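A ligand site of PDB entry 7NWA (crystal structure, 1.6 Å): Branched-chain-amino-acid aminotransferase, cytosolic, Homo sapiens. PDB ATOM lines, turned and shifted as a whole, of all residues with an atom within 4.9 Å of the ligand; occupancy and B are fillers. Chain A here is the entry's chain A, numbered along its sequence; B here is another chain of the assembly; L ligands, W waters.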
ATOM      1  N   PHE A  52     -20.755  -0.504  13.820  1.00  0.00           N
ATOM      2  CA  PHE A  52     -21.135  -1.106  15.113  1.00  0.00           C
ATOM      3  C   PHE A  52     -22.503  -1.804  15.002  1.00  0.00           C
ATOM      4  O   PHE A  52     -23.467  -1.217  14.520  1.00  0.00           O
ATOM      5  CB  PHE A  52     -21.213  -0.059  16.230  1.00  0.00           C
ATOM      6  CG  PHE A  52     -21.695  -0.674  17.516  1.00  0.00           C
ATOM      7  CD1 PHE A  52     -20.846  -1.488  18.275  1.00  0.00           C
ATOM      8  CD2 PHE A  52     -23.013  -0.555  17.915  1.00  0.00           C
ATOM      9  CE1 PHE A  52     -21.316  -2.092  19.426  1.00  0.00           C
ATOM     10  CE2 PHE A  52     -23.469  -1.137  19.087  1.00  0.00           C
ATOM     11  CZ  PHE A  52     -22.627  -1.923  19.817  1.00  0.00           C
ATOM     12  N   PHE A  98     -30.755  -6.291  28.563  1.00  0.00           N
ATOM     13  CA  PHE A  98     -29.618  -6.698  27.721  1.00  0.00           C
ATOM     14  C   PHE A  98     -28.315  -6.382  28.421  1.00  0.00           C
ATOM     15  O   PHE A  98     -28.294  -5.674  29.462  1.00  0.00           O
ATOM     16  CB  PHE A  98     -29.682  -5.998  26.353  1.00  0.00           C
ATOM     17  CG  PHE A  98     -29.416  -4.520  26.423  1.00  0.00           C
ATOM     18  CD1 PHE A  98     -30.462  -3.634  26.701  1.00  0.00           C
ATOM     19  CD2 PHE A  98     -28.169  -4.003  26.153  1.00  0.00           C
ATOM     20  CE1 PHE A  98     -30.228  -2.279  26.778  1.00  0.00           C
ATOM     21  CE2 PHE A  98     -27.947  -2.633  26.186  1.00  0.00           C
ATOM     22  CZ  PHE A  98     -28.975  -1.782  26.501  1.00  0.00           C
ATOM     23  N   TYR A 164     -18.369  -7.999  19.605  1.00  0.00           N
ATOM     24  CA  TYR A 164     -19.390  -7.531  20.557  1.00  0.00           C
ATOM     25  C   TYR A 164     -20.326  -8.688  20.862  1.00  0.00           C
ATOM     26  O   TYR A 164     -20.741  -9.400  19.939  1.00  0.00           O
ATOM     27  CB  TYR A 164     -20.142  -6.327  19.997  1.00  0.00           C
ATOM     28  CG  TYR A 164     -21.072  -5.654  20.980  1.00  0.00           C
ATOM     29  CD1 TYR A 164     -20.604  -4.838  21.994  1.00  0.00           C
ATOM     30  CD2 TYR A 164     -22.444  -5.810  20.859  1.00  0.00           C
ATOM     31  CE1 TYR A 164     -21.469  -4.201  22.865  1.00  0.00           C
ATOM     32  CE2 TYR A 164     -23.318  -5.202  21.732  1.00  0.00           C
ATOM     33  CZ  TYR A 164     -22.841  -4.358  22.721  1.00  0.00           C
ATOM     34  OH  TYR A 164     -23.693  -3.760  23.599  1.00  0.00           O
ATOM     35  N   ARG A 166     -23.845  -9.697  22.842  1.00  0.00           N
ATOM     36  CA  ARG A 166     -25.135  -9.098  23.247  1.00  0.00           C
ATOM     37  C   ARG A 166     -26.025 -10.167  23.859  1.00  0.00           C
ATOM     38  O   ARG A 166     -26.873 -10.749  23.190  1.00  0.00           O
ATOM     39  CB  ARG A 166     -25.755  -8.415  22.020  1.00  0.00           C
ATOM     40  CG  ARG A 166     -27.200  -7.952  22.173  1.00  0.00           C
ATOM     41  CD  ARG A 166     -27.530  -7.126  23.422  1.00  0.00           C
ATOM     42  NE  ARG A 166     -26.797  -5.853  23.429  1.00  0.00           N
ATOM     43  CZ  ARG A 166     -27.248  -4.692  22.913  1.00  0.00           C
ATOM     44  NH1 ARG A 166     -28.424  -4.615  22.338  1.00  0.00           N
ATOM     45  NH2 ARG A 166     -26.511  -3.588  22.984  1.00  0.00           N
ATOM     46  N   TYR A 196     -15.780   2.528  17.296  1.00  0.00           N
ATOM     47  CA  TYR A 196     -17.144   3.097  17.216  1.00  0.00           C
ATOM     48  C   TYR A 196     -17.195   4.079  16.028  1.00  0.00           C
ATOM     49  O   TYR A 196     -18.169   4.009  15.255  1.00  0.00           O
ATOM     50  CB  TYR A 196     -17.604   3.734  18.529  1.00  0.00           C
ATOM     51  CG  TYR A 196     -19.003   4.270  18.430  1.00  0.00           C
ATOM     52  CD1 TYR A 196     -20.109   3.431  18.460  1.00  0.00           C
ATOM     53  CD2 TYR A 196     -19.213   5.619  18.201  1.00  0.00           C
ATOM     54  CE1 TYR A 196     -21.390   3.929  18.305  1.00  0.00           C
ATOM     55  CE2 TYR A 196     -20.489   6.130  18.006  1.00  0.00           C
ATOM     56  CZ  TYR A 196     -21.576   5.280  18.076  1.00  0.00           C
ATOM     57  OH  TYR A 196     -22.835   5.791  17.907  1.00  0.00           O
ATOM     58  N   PHE A 197     -16.182   4.951  15.882  1.00  0.00           N
ATOM     59  CA  PHE A 197     -16.069   5.915  14.750  1.00  0.00           C
ATOM     60  C   PHE A 197     -15.122   5.363  13.674  1.00  0.00           C
ATOM     61  O   PHE A 197     -14.034   4.890  14.038  1.00  0.00           O
ATOM     62  CB  PHE A 197     -15.620   7.299  15.246  1.00  0.00           C
ATOM     63  CG  PHE A 197     -16.696   8.039  16.000  1.00  0.00           C
ATOM     64  CD1 PHE A 197     -17.800   8.570  15.337  1.00  0.00           C
ATOM     65  CD2 PHE A 197     -16.603   8.236  17.366  1.00  0.00           C
ATOM     66  CE1 PHE A 197     -18.783   9.257  16.029  1.00  0.00           C
ATOM     67  CE2 PHE A 197     -17.581   8.949  18.047  1.00  0.00           C
ATOM     68  CZ  PHE A 197     -18.664   9.446  17.386  1.00  0.00           C
ATOM     69  N   VAL A 205     -17.672  15.175  20.137  1.00  0.00           N
ATOM     70  CA  VAL A 205     -19.099  15.452  19.812  1.00  0.00           C
ATOM     71  C   VAL A 205     -19.572  16.746  20.449  1.00  0.00           C
ATOM     72  O   VAL A 205     -19.040  17.162  21.504  1.00  0.00           O
ATOM     73  CB  VAL A 205     -20.028  14.294  20.229  1.00  0.00           C
ATOM     74  CG1 VAL A 205     -19.832  13.093  19.324  1.00  0.00           C
ATOM     75  CG2 VAL A 205     -19.843  13.958  21.687  1.00  0.00           C
ATOM     76  N   LEU A 207     -22.966  18.314  22.225  1.00  0.00           N
ATOM     77  CA  LEU A 207     -24.093  17.787  23.017  1.00  0.00           C
ATOM     78  C   LEU A 207     -25.223  18.808  23.015  1.00  0.00           C
ATOM     79  O   LEU A 207     -24.955  19.999  23.106  1.00  0.00           O
ATOM     80  CB  LEU A 207     -23.645  17.522  24.455  1.00  0.00           C
ATOM     81  CG  LEU A 207     -22.446  16.594  24.602  1.00  0.00           C
ATOM     82  CD1 LEU A 207     -22.157  16.402  26.081  1.00  0.00           C
ATOM     83  CD2 LEU A 207     -22.658  15.269  23.894  1.00  0.00           C
ATOM     84  N   LYS A 225     -29.899  -2.191  33.120  1.00  0.00           N
ATOM     85  CA  LYS A 225     -29.816  -2.176  31.638  1.00  0.00           C
ATOM     86  C   LYS A 225     -31.104  -2.788  31.094  1.00  0.00           C
ATOM     87  O   LYS A 225     -31.065  -3.826  30.452  1.00  0.00           O
ATOM     88  CB  LYS A 225     -28.544  -2.892  31.187  1.00  0.00           C
ATOM     89  CG  LYS A 225     -27.702  -2.086  30.234  1.00  0.00           C
ATOM     90  CD  LYS A 225     -26.351  -2.632  29.967  1.00  0.00           C
ATOM     91  CE  LYS A 225     -25.735  -2.028  28.736  1.00  0.00           C
ATOM     92  NZ  LYS A 225     -25.741  -0.538  28.722  1.00  0.00           N
ATOM     93  N   TYR A 230     -34.646   3.263  27.201  1.00  0.00           N
ATOM     94  CA  TYR A 230     -33.955   3.667  25.976  1.00  0.00           C
ATOM     95  C   TYR A 230     -34.913   4.093  24.922  1.00  0.00           C
ATOM     96  O   TYR A 230     -34.539   4.804  24.058  1.00  0.00           O
ATOM     97  CB  TYR A 230     -33.036   2.566  25.401  1.00  0.00           C
ATOM     98  CG  TYR A 230     -31.907   2.211  26.294  1.00  0.00           C
ATOM     99  CD1 TYR A 230     -32.053   1.266  27.229  1.00  0.00           C
ATOM    100  CD2 TYR A 230     -30.702   2.827  26.185  1.00  0.00           C
ATOM    101  CE1 TYR A 230     -31.052   0.961  28.087  1.00  0.00           C
ATOM    102  CE2 TYR A 230     -29.696   2.500  27.013  1.00  0.00           C
ATOM    103  CZ  TYR A 230     -29.869   1.539  27.954  1.00  0.00           C
ATOM    104  OH  TYR A 230     -28.853   1.244  28.824  1.00  0.00           O
ATOM    105  N   GLN A 247     -25.180  14.216  20.056  1.00  0.00           N
ATOM    106  CA  GLN A 247     -25.615  13.402  21.224  1.00  0.00           C
ATOM    107  C   GLN A 247     -26.357  14.278  22.225  1.00  0.00           C
ATOM    108  O   GLN A 247     -26.219  15.525  22.164  1.00  0.00           O
ATOM    109  CB  GLN A 247     -24.417  12.765  21.922  1.00  0.00           C
ATOM    110  CG  GLN A 247     -23.628  11.795  21.055  1.00  0.00           C
ATOM    111  CD  GLN A 247     -24.393  10.536  20.725  1.00  0.00           C
ATOM    112  OE1 GLN A 247     -25.236  10.068  21.479  1.00  0.00           O
ATOM    113  NE2 GLN A 247     -24.063   9.935  19.588  1.00  0.00           N
ATOM    114  N   VAL A 261     -24.385  10.960  28.905  1.00  0.00           N
ATOM    115  CA  VAL A 261     -24.255  11.577  27.565  1.00  0.00           C
ATOM    116  C   VAL A 261     -24.574  10.477  26.560  1.00  0.00           C
ATOM    117  O   VAL A 261     -23.884   9.452  26.528  1.00  0.00           O
ATOM    118  CB  VAL A 261     -22.901  12.276  27.394  1.00  0.00           C
ATOM    119  CG1 VAL A 261     -21.727  11.377  27.727  1.00  0.00           C
ATOM    120  CG2 VAL A 261     -22.725  12.884  26.035  1.00  0.00           C
ATOM    121  N   GLY A 262     -25.645  10.664  25.796  1.00  0.00           N
ATOM    122  CA  GLY A 262     -26.195   9.587  24.961  1.00  0.00           C
ATOM    123  C   GLY A 262     -26.407   8.344  25.804  1.00  0.00           C
ATOM    124  O   GLY A 262     -27.068   8.436  26.868  1.00  0.00           O
ATOM    125  N   THR A 263     -25.828   7.204  25.401  1.00  0.00           N
ATOM    126  CA  THR A 263     -25.900   5.921  26.121  1.00  0.00           C
ATOM    127  C   THR A 263     -24.641   5.684  26.950  1.00  0.00           C
ATOM    128  O   THR A 263     -24.381   4.530  27.278  1.00  0.00           O
ATOM    129  CB  THR A 263     -26.055   4.755  25.129  1.00  0.00           C
ATOM    130  OG1 THR A 263     -24.926   4.805  24.259  1.00  0.00           O
ATOM    131  CG2 THR A 263     -27.333   4.831  24.337  1.00  0.00           C
ATOM    132  N   MET A 264     -23.890   6.727  27.276  1.00  0.00           N
ATOM    133  CA  MET A 264     -22.561   6.592  27.913  1.00  0.00           C
ATOM    134  C   MET A 264     -22.557   7.316  29.268  1.00  0.00           C
ATOM    135  O   MET A 264     -23.308   8.300  29.456  1.00  0.00           O
ATOM    136  CB  MET A 264     -21.480   7.203  27.001  1.00  0.00           C
ATOM    137  CG  MET A 264     -21.361   6.447  25.668  1.00  0.00           C
ATOM    138  SD  MET A 264     -19.989   7.072  24.649  1.00  0.00           S
ATOM    139  CE  MET A 264     -18.610   6.218  25.401  1.00  0.00           C
ATOM    140  N   GLY A 333     -17.362  10.791  27.458  1.00  0.00           N
ATOM    141  CA  GLY A 333     -18.247   9.652  27.756  1.00  0.00           C
ATOM    142  C   GLY A 333     -17.439   8.382  27.920  1.00  0.00           C
ATOM    143  O   GLY A 333     -16.355   8.266  27.285  1.00  0.00           O
ATOM    144  N   GLY A 335     -18.052   3.976  27.777  1.00  0.00           N
ATOM    145  CA  GLY A 335     -18.982   2.876  27.450  1.00  0.00           C
ATOM    146  C   GLY A 335     -18.294   1.826  26.622  1.00  0.00           C
ATOM    147  O   GLY A 335     -17.227   2.099  26.090  1.00  0.00           O
ATOM    148  N   THR A 336     -18.890   0.651  26.485  1.00  0.00           N
ATOM    149  CA  THR A 336     -18.243  -0.508  25.826  1.00  0.00           C
ATOM    150  C   THR A 336     -17.991  -0.232  24.341  1.00  0.00           C
ATOM    151  O   THR A 336     -16.856  -0.496  23.880  1.00  0.00           O
ATOM    152  CB  THR A 336     -19.070  -1.778  26.081  1.00  0.00           C
ATOM    153  OG1 THR A 336     -18.988  -2.013  27.487  1.00  0.00           O
ATOM    154  CG2 THR A 336     -18.580  -2.964  25.297  1.00  0.00           C
ATOM    155  N   ALA A 337     -18.987   0.265  23.593  1.00  0.00           N
ATOM    156  CA  ALA A 337     -18.843   0.398  22.125  1.00  0.00           C
ATOM    157  C   ALA A 337     -17.767   1.437  21.792  1.00  0.00           C
ATOM    158  O   ALA A 337     -17.019   1.215  20.832  1.00  0.00           O
ATOM    159  CB  ALA A 337     -20.169   0.708  21.477  1.00  0.00           C
ATOM    160  N   CYS A 338     -17.658   2.542  22.538  1.00  0.00           N
ATOM    161  CA  CYS A 338     -16.726   3.648  22.183  1.00  0.00           C
ATOM    162  C   CYS A 338     -15.450   3.689  23.053  1.00  0.00           C
ATOM    163  O   CYS A 338     -14.416   4.211  22.560  1.00  0.00           O
ATOM    164  CB  CYS A 338     -17.406   5.015  22.238  1.00  0.00           C
ATOM    165  SG  CYS A 338     -16.179   6.349  22.108  1.00  0.00           S
ATOM    166  N   VAL A 339     -15.509   3.131  24.249  1.00  0.00           N
ATOM    167  CA  VAL A 339     -14.508   3.128  25.366  1.00  0.00           C
ATOM    168  C   VAL A 339     -14.446   4.524  25.984  1.00  0.00           C
ATOM    169  O   VAL A 339     -14.986   4.688  27.095  1.00  0.00           O
ATOM    170  CB  VAL A 339     -13.104   2.630  24.979  1.00  0.00           C
ATOM    171  CG1 VAL A 339     -12.264   2.482  26.231  1.00  0.00           C
ATOM    172  CG2 VAL A 339     -13.136   1.324  24.181  1.00  0.00           C
ATOM    173  N   CYS A 341     -15.103   8.622  24.695  1.00  0.00           N
ATOM    174  CA  CYS A 341     -15.659   9.476  23.613  1.00  0.00           C
ATOM    175  C   CYS A 341     -15.622  10.930  24.039  1.00  0.00           C
ATOM    176  O   CYS A 341     -16.466  11.377  24.800  1.00  0.00           O
ATOM    177  CB  CYS A 341     -17.089   9.068  23.266  1.00  0.00           C
ATOM    178  SG  CYS A 341     -17.271   8.037  21.783  1.00  0.00           S
ATOM    179  N   PRO A 342     -14.610  11.732  23.629  1.00  0.00           N
ATOM    180  CA  PRO A 342     -14.529  13.120  24.067  1.00  0.00           C
ATOM    181  C   PRO A 342     -15.668  14.022  23.624  1.00  0.00           C
ATOM    182  O   PRO A 342     -16.273  13.785  22.570  1.00  0.00           O
ATOM    183  CB  PRO A 342     -13.232  13.637  23.428  1.00  0.00           C
ATOM    184  CG  PRO A 342     -12.406  12.372  23.237  1.00  0.00           C
ATOM    185  CD  PRO A 342     -13.425  11.321  22.857  1.00  0.00           C
ATOM    186  N   VAL A 343     -15.910  15.043  24.447  1.00  0.00           N
ATOM    187  CA  VAL A 343     -16.929  16.106  24.207  1.00  0.00           C
ATOM    188  C   VAL A 343     -16.214  17.424  23.921  1.00  0.00           C
ATOM    189  O   VAL A 343     -15.368  17.827  24.740  1.00  0.00           O
ATOM    190  CB  VAL A 343     -17.858  16.211  25.417  1.00  0.00           C
ATOM    191  CG1 VAL A 343     -18.792  17.399  25.293  1.00  0.00           C
ATOM    192  CG2 VAL A 343     -18.616  14.900  25.641  1.00  0.00           C
ATOM    193  N   TYR B  93     -34.316  -2.072  23.057  1.00  0.00           N
ATOM    194  CA  TYR B  93     -34.439  -0.653  23.489  1.00  0.00           C
ATOM    195  C   TYR B  93     -35.911  -0.234  23.542  1.00  0.00           C
ATOM    196  O   TYR B  93     -36.202   0.975  23.557  1.00  0.00           O
ATOM    197  CB  TYR B  93     -33.618   0.245  22.562  1.00  0.00           C
ATOM    198  CG  TYR B  93     -32.209  -0.231  22.304  1.00  0.00           C
ATOM    199  CD1 TYR B  93     -31.387  -0.585  23.353  1.00  0.00           C
ATOM    200  CD2 TYR B  93     -31.749  -0.427  21.022  1.00  0.00           C
ATOM    201  CE1 TYR B  93     -30.106  -1.077  23.126  1.00  0.00           C
ATOM    202  CE2 TYR B  93     -30.469  -0.921  20.773  1.00  0.00           C
ATOM    203  CZ  TYR B  93     -29.638  -1.234  21.828  1.00  0.00           C
ATOM    204  OH  TYR B  93     -28.384  -1.720  21.566  1.00  0.00           O
ATOM    205  N   LEU B 176     -27.750  -2.933  16.339  1.00  0.00           N
ATOM    206  CA  LEU B 176     -27.763  -2.746  17.816  1.00  0.00           C
ATOM    207  C   LEU B 176     -27.478  -1.289  18.182  1.00  0.00           C
ATOM    208  O   LEU B 176     -27.469  -0.975  19.377  1.00  0.00           O
ATOM    209  CB  LEU B 176     -26.753  -3.692  18.448  1.00  0.00           C
ATOM    210  CG  LEU B 176     -26.933  -5.168  18.107  1.00  0.00           C
ATOM    211  CD1 LEU B 176     -25.911  -5.986  18.865  1.00  0.00           C
ATOM    212  CD2 LEU B 176     -28.330  -5.654  18.414  1.00  0.00           C
ATOM    213  N   GLY B 177     -27.195  -0.404  17.224  1.00  0.00           N
ATOM    214  CA  GLY B 177     -27.091   1.016  17.584  1.00  0.00           C
ATOM    215  C   GLY B 177     -28.416   1.520  18.116  1.00  0.00           C
ATOM    216  O   GLY B 177     -29.503   1.084  17.628  1.00  0.00           O
ATOM    217  N   VAL B 178     -28.385   2.416  19.092  1.00  0.00           N
ATOM    218  CA  VAL B 178     -29.612   3.047  19.641  1.00  0.00           C
ATOM    219  C   VAL B 178     -29.942   4.165  18.667  1.00  0.00           C
ATOM    220  O   VAL B 178     -29.276   5.227  18.716  1.00  0.00           O
ATOM    221  CB  VAL B 178     -29.430   3.520  21.096  1.00  0.00           C
ATOM    222  CG1 VAL B 178     -30.685   4.202  21.606  1.00  0.00           C
ATOM    223  CG2 VAL B 178     -29.046   2.374  22.029  1.00  0.00           C
HETATM  224  N1  LIG L   1     -24.035   3.509  21.285  1.00  0.00           N
HETATM  225  C1  LIG L   1     -22.508   4.939  21.719  1.00  0.00           C
HETATM  226  C2  LIG L   1     -22.438   7.332  20.990  1.00  0.00           C
HETATM  227  C3  LIG L   1     -21.868   8.488  21.802  1.00  0.00           C
HETATM  228  C4  LIG L   1     -21.858   9.792  23.842  1.00  0.00           C
HETATM  229  C5  LIG L   1     -20.792   9.209  21.341  1.00  0.00           C
HETATM  230  C6  LIG L   1     -25.130   2.802  20.796  1.00  0.00           C
HETATM  231  C7  LIG L   1     -24.782  -0.413  22.788  1.00  0.00           C
HETATM  232  C8  LIG L   1     -25.286  -0.294  24.219  1.00  0.00           C
HETATM  233  N2  LIG L   1     -20.325   3.451  24.205  1.00  0.00           N
HETATM  234  C9  LIG L   1     -21.153   3.641  23.453  1.00  0.00           C
HETATM  235  C10 LIG L   1     -22.226   3.831  22.528  1.00  0.00           C
HETATM  236  C11 LIG L   1     -23.196   2.895  22.260  1.00  0.00           C
HETATM  237  N3  LIG L   1     -23.441   1.661  22.713  1.00  0.00           N
HETATM  238  C12 LIG L   1     -24.499   0.954  22.241  1.00  0.00           C
HETATM  239  C13 LIG L   1     -26.541   0.558  24.387  1.00  0.00           C
HETATM  240  C14 LIG L   1     -25.370   1.515  21.274  1.00  0.00           C
HETATM  241  O1  LIG L   1     -25.833   3.361  19.924  1.00  0.00           O
HETATM  242  N4  LIG L   1     -23.605   4.650  21.017  1.00  0.00           N
HETATM  243  N5  LIG L   1     -21.848   6.095  21.637  1.00  0.00           N
HETATM  244  C15 LIG L   1     -22.397   8.782  23.061  1.00  0.00           C
HETATM  245  F1  LIG L   1     -23.436   8.106  23.537  1.00  0.00           F
HETATM  246  C16 LIG L   1     -20.764  10.487  23.346  1.00  0.00           C
HETATM  247 CL1  LIG L   1     -20.041  11.717  24.316  1.00  0.00          CL
HETATM  248  C17 LIG L   1     -20.222  10.224  22.094  1.00  0.00           C
HETATM  249  F2  LIG L   1     -20.255   8.922  20.121  1.00  0.00           F
HETATM  250  O   HOH W   1     -22.392   2.303  26.685  1.00  0.00           O
HETATM  251  O   HOH W   2     -26.286   7.530  22.152  1.00  0.00           O
HETATM  252  O   HOH W   3     -24.912   4.189  17.430  1.00  0.00           O
HETATM  253  O   HOH W   4     -22.562  -2.099  25.262  1.00  0.00           O
HETATM  254  O   HOH W   5     -26.761   5.902  19.951  1.00  0.00           O
HETATM  255  O   HOH W   6     -21.748   0.511  24.630  1.00  0.00           O
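The backbone NH (N) of Val 178 of chain B is in hydrogen-bond range of an oxygen (O1) of the ligand (2.8 Å). A nitrogen (N2) of the ligand sits at hydrogen-bond distance from the backbone NH of Cys 338, 3.3 Å away. The side-chain sulfur of Met 264 lies close to a nitrogen (N5) of the ligand (3.7 Å). The side-chain hydroxyl (OH) of Tyr 196 lies within hydrogen-bond range of a nitrogen (N4) of the ligand (3.4 Å).
SG of Cys 338 forms a disulfide with SG of Cys 341 (2.0 Å). N of Val 205 is in hydrogen-bond range of O of Pro 342 (3.1 Å). The backbone carbonyl oxygen of Cys 341 is in hydrogen-bond range of the backbone NH of Gly 333. The guanidinium group of Arg 166 is in hydrogen-bond range of the side-chain hydroxyl of Tyr 164 (2.9 Å). The side-chain hydroxyl (OH) of Tyr 93 of chain B is in hydrogen-bond range of the guanidinium group (NH1) of Arg 166 (3.0 Å). The backbone carbonyl oxygen (O) of Leu 176 of chain B sits at hydrogen-bond distance from the side-chain hydroxyl (OH) of Tyr 93 of chain B (2.5 Å). N of Phe 98 lies within hydrogen-bond range of O of Lys 225 (3.1 Å).
The side-chain amide oxygen of Gln 247 sits close to a fluorine (F1) of the ligand, at 3.4 Å. O of Val 261 sits close to F1 of the ligand, 3.3 Å away. N of Thr 263 sits close to F1 of the ligand. The side-chain sulfur (SG) of Cys 341 lies close to a fluorine (F2) of the ligand (3.5 Å). Merely in contact with the ligand: Phe 197 (3.2 Å), Gly 262 (3.4 Å), Val 205 (3.5 Å), Ala 337 (3.5 Å), Gly 177 of chain B (3.5 Å), Gly 335 (3.6 Å), Tyr 164 (3.6 Å), Arg 166 (3.6 Å), Val 343 (3.7 Å), Leu 176 of chain B (3.8 Å), Thr 336 (3.9 Å), Phe 52 (3.9 Å) and Phe 98 (3.9 Å). Hydrophobic or aromatic side chains that line the ligand: Phe 52, Phe 98, Tyr 196, Phe 197, Val 205, Val 261, Met 264, Ala 337, Val 343 and Val 178 of chain B. Within 4 Å of the ligand: Phe 52, Phe 98, Tyr 164, Arg 166, Tyr 196, Phe 197, Val 205, Gln 247, Val 261, Gly 262, Thr 263, Met 264, Gly 335, Thr 336, Ala 337, Cys 338, Cys 341, Val 343, Leu 176 of chain B, Gly 177 of chain B and Val 178 of chain B. The nearest printed residue that does not touch the ligand is Tyr 93 of chain B (4.02 Å).
Water W5 bridges O1 of the ligand (2.7 Å) and O of Val 178 of chain B (2.9 Å). Water W3 lies within hydrogen-bond range of OH of Tyr 196 and O1 of the ligand. Water W2 bridges the side-chain amide oxygen (OE1) of Gln 247 and the backbone NH (N) of Thr 263. Water W1 bridges O of Thr 263 and N2 of the ligand.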
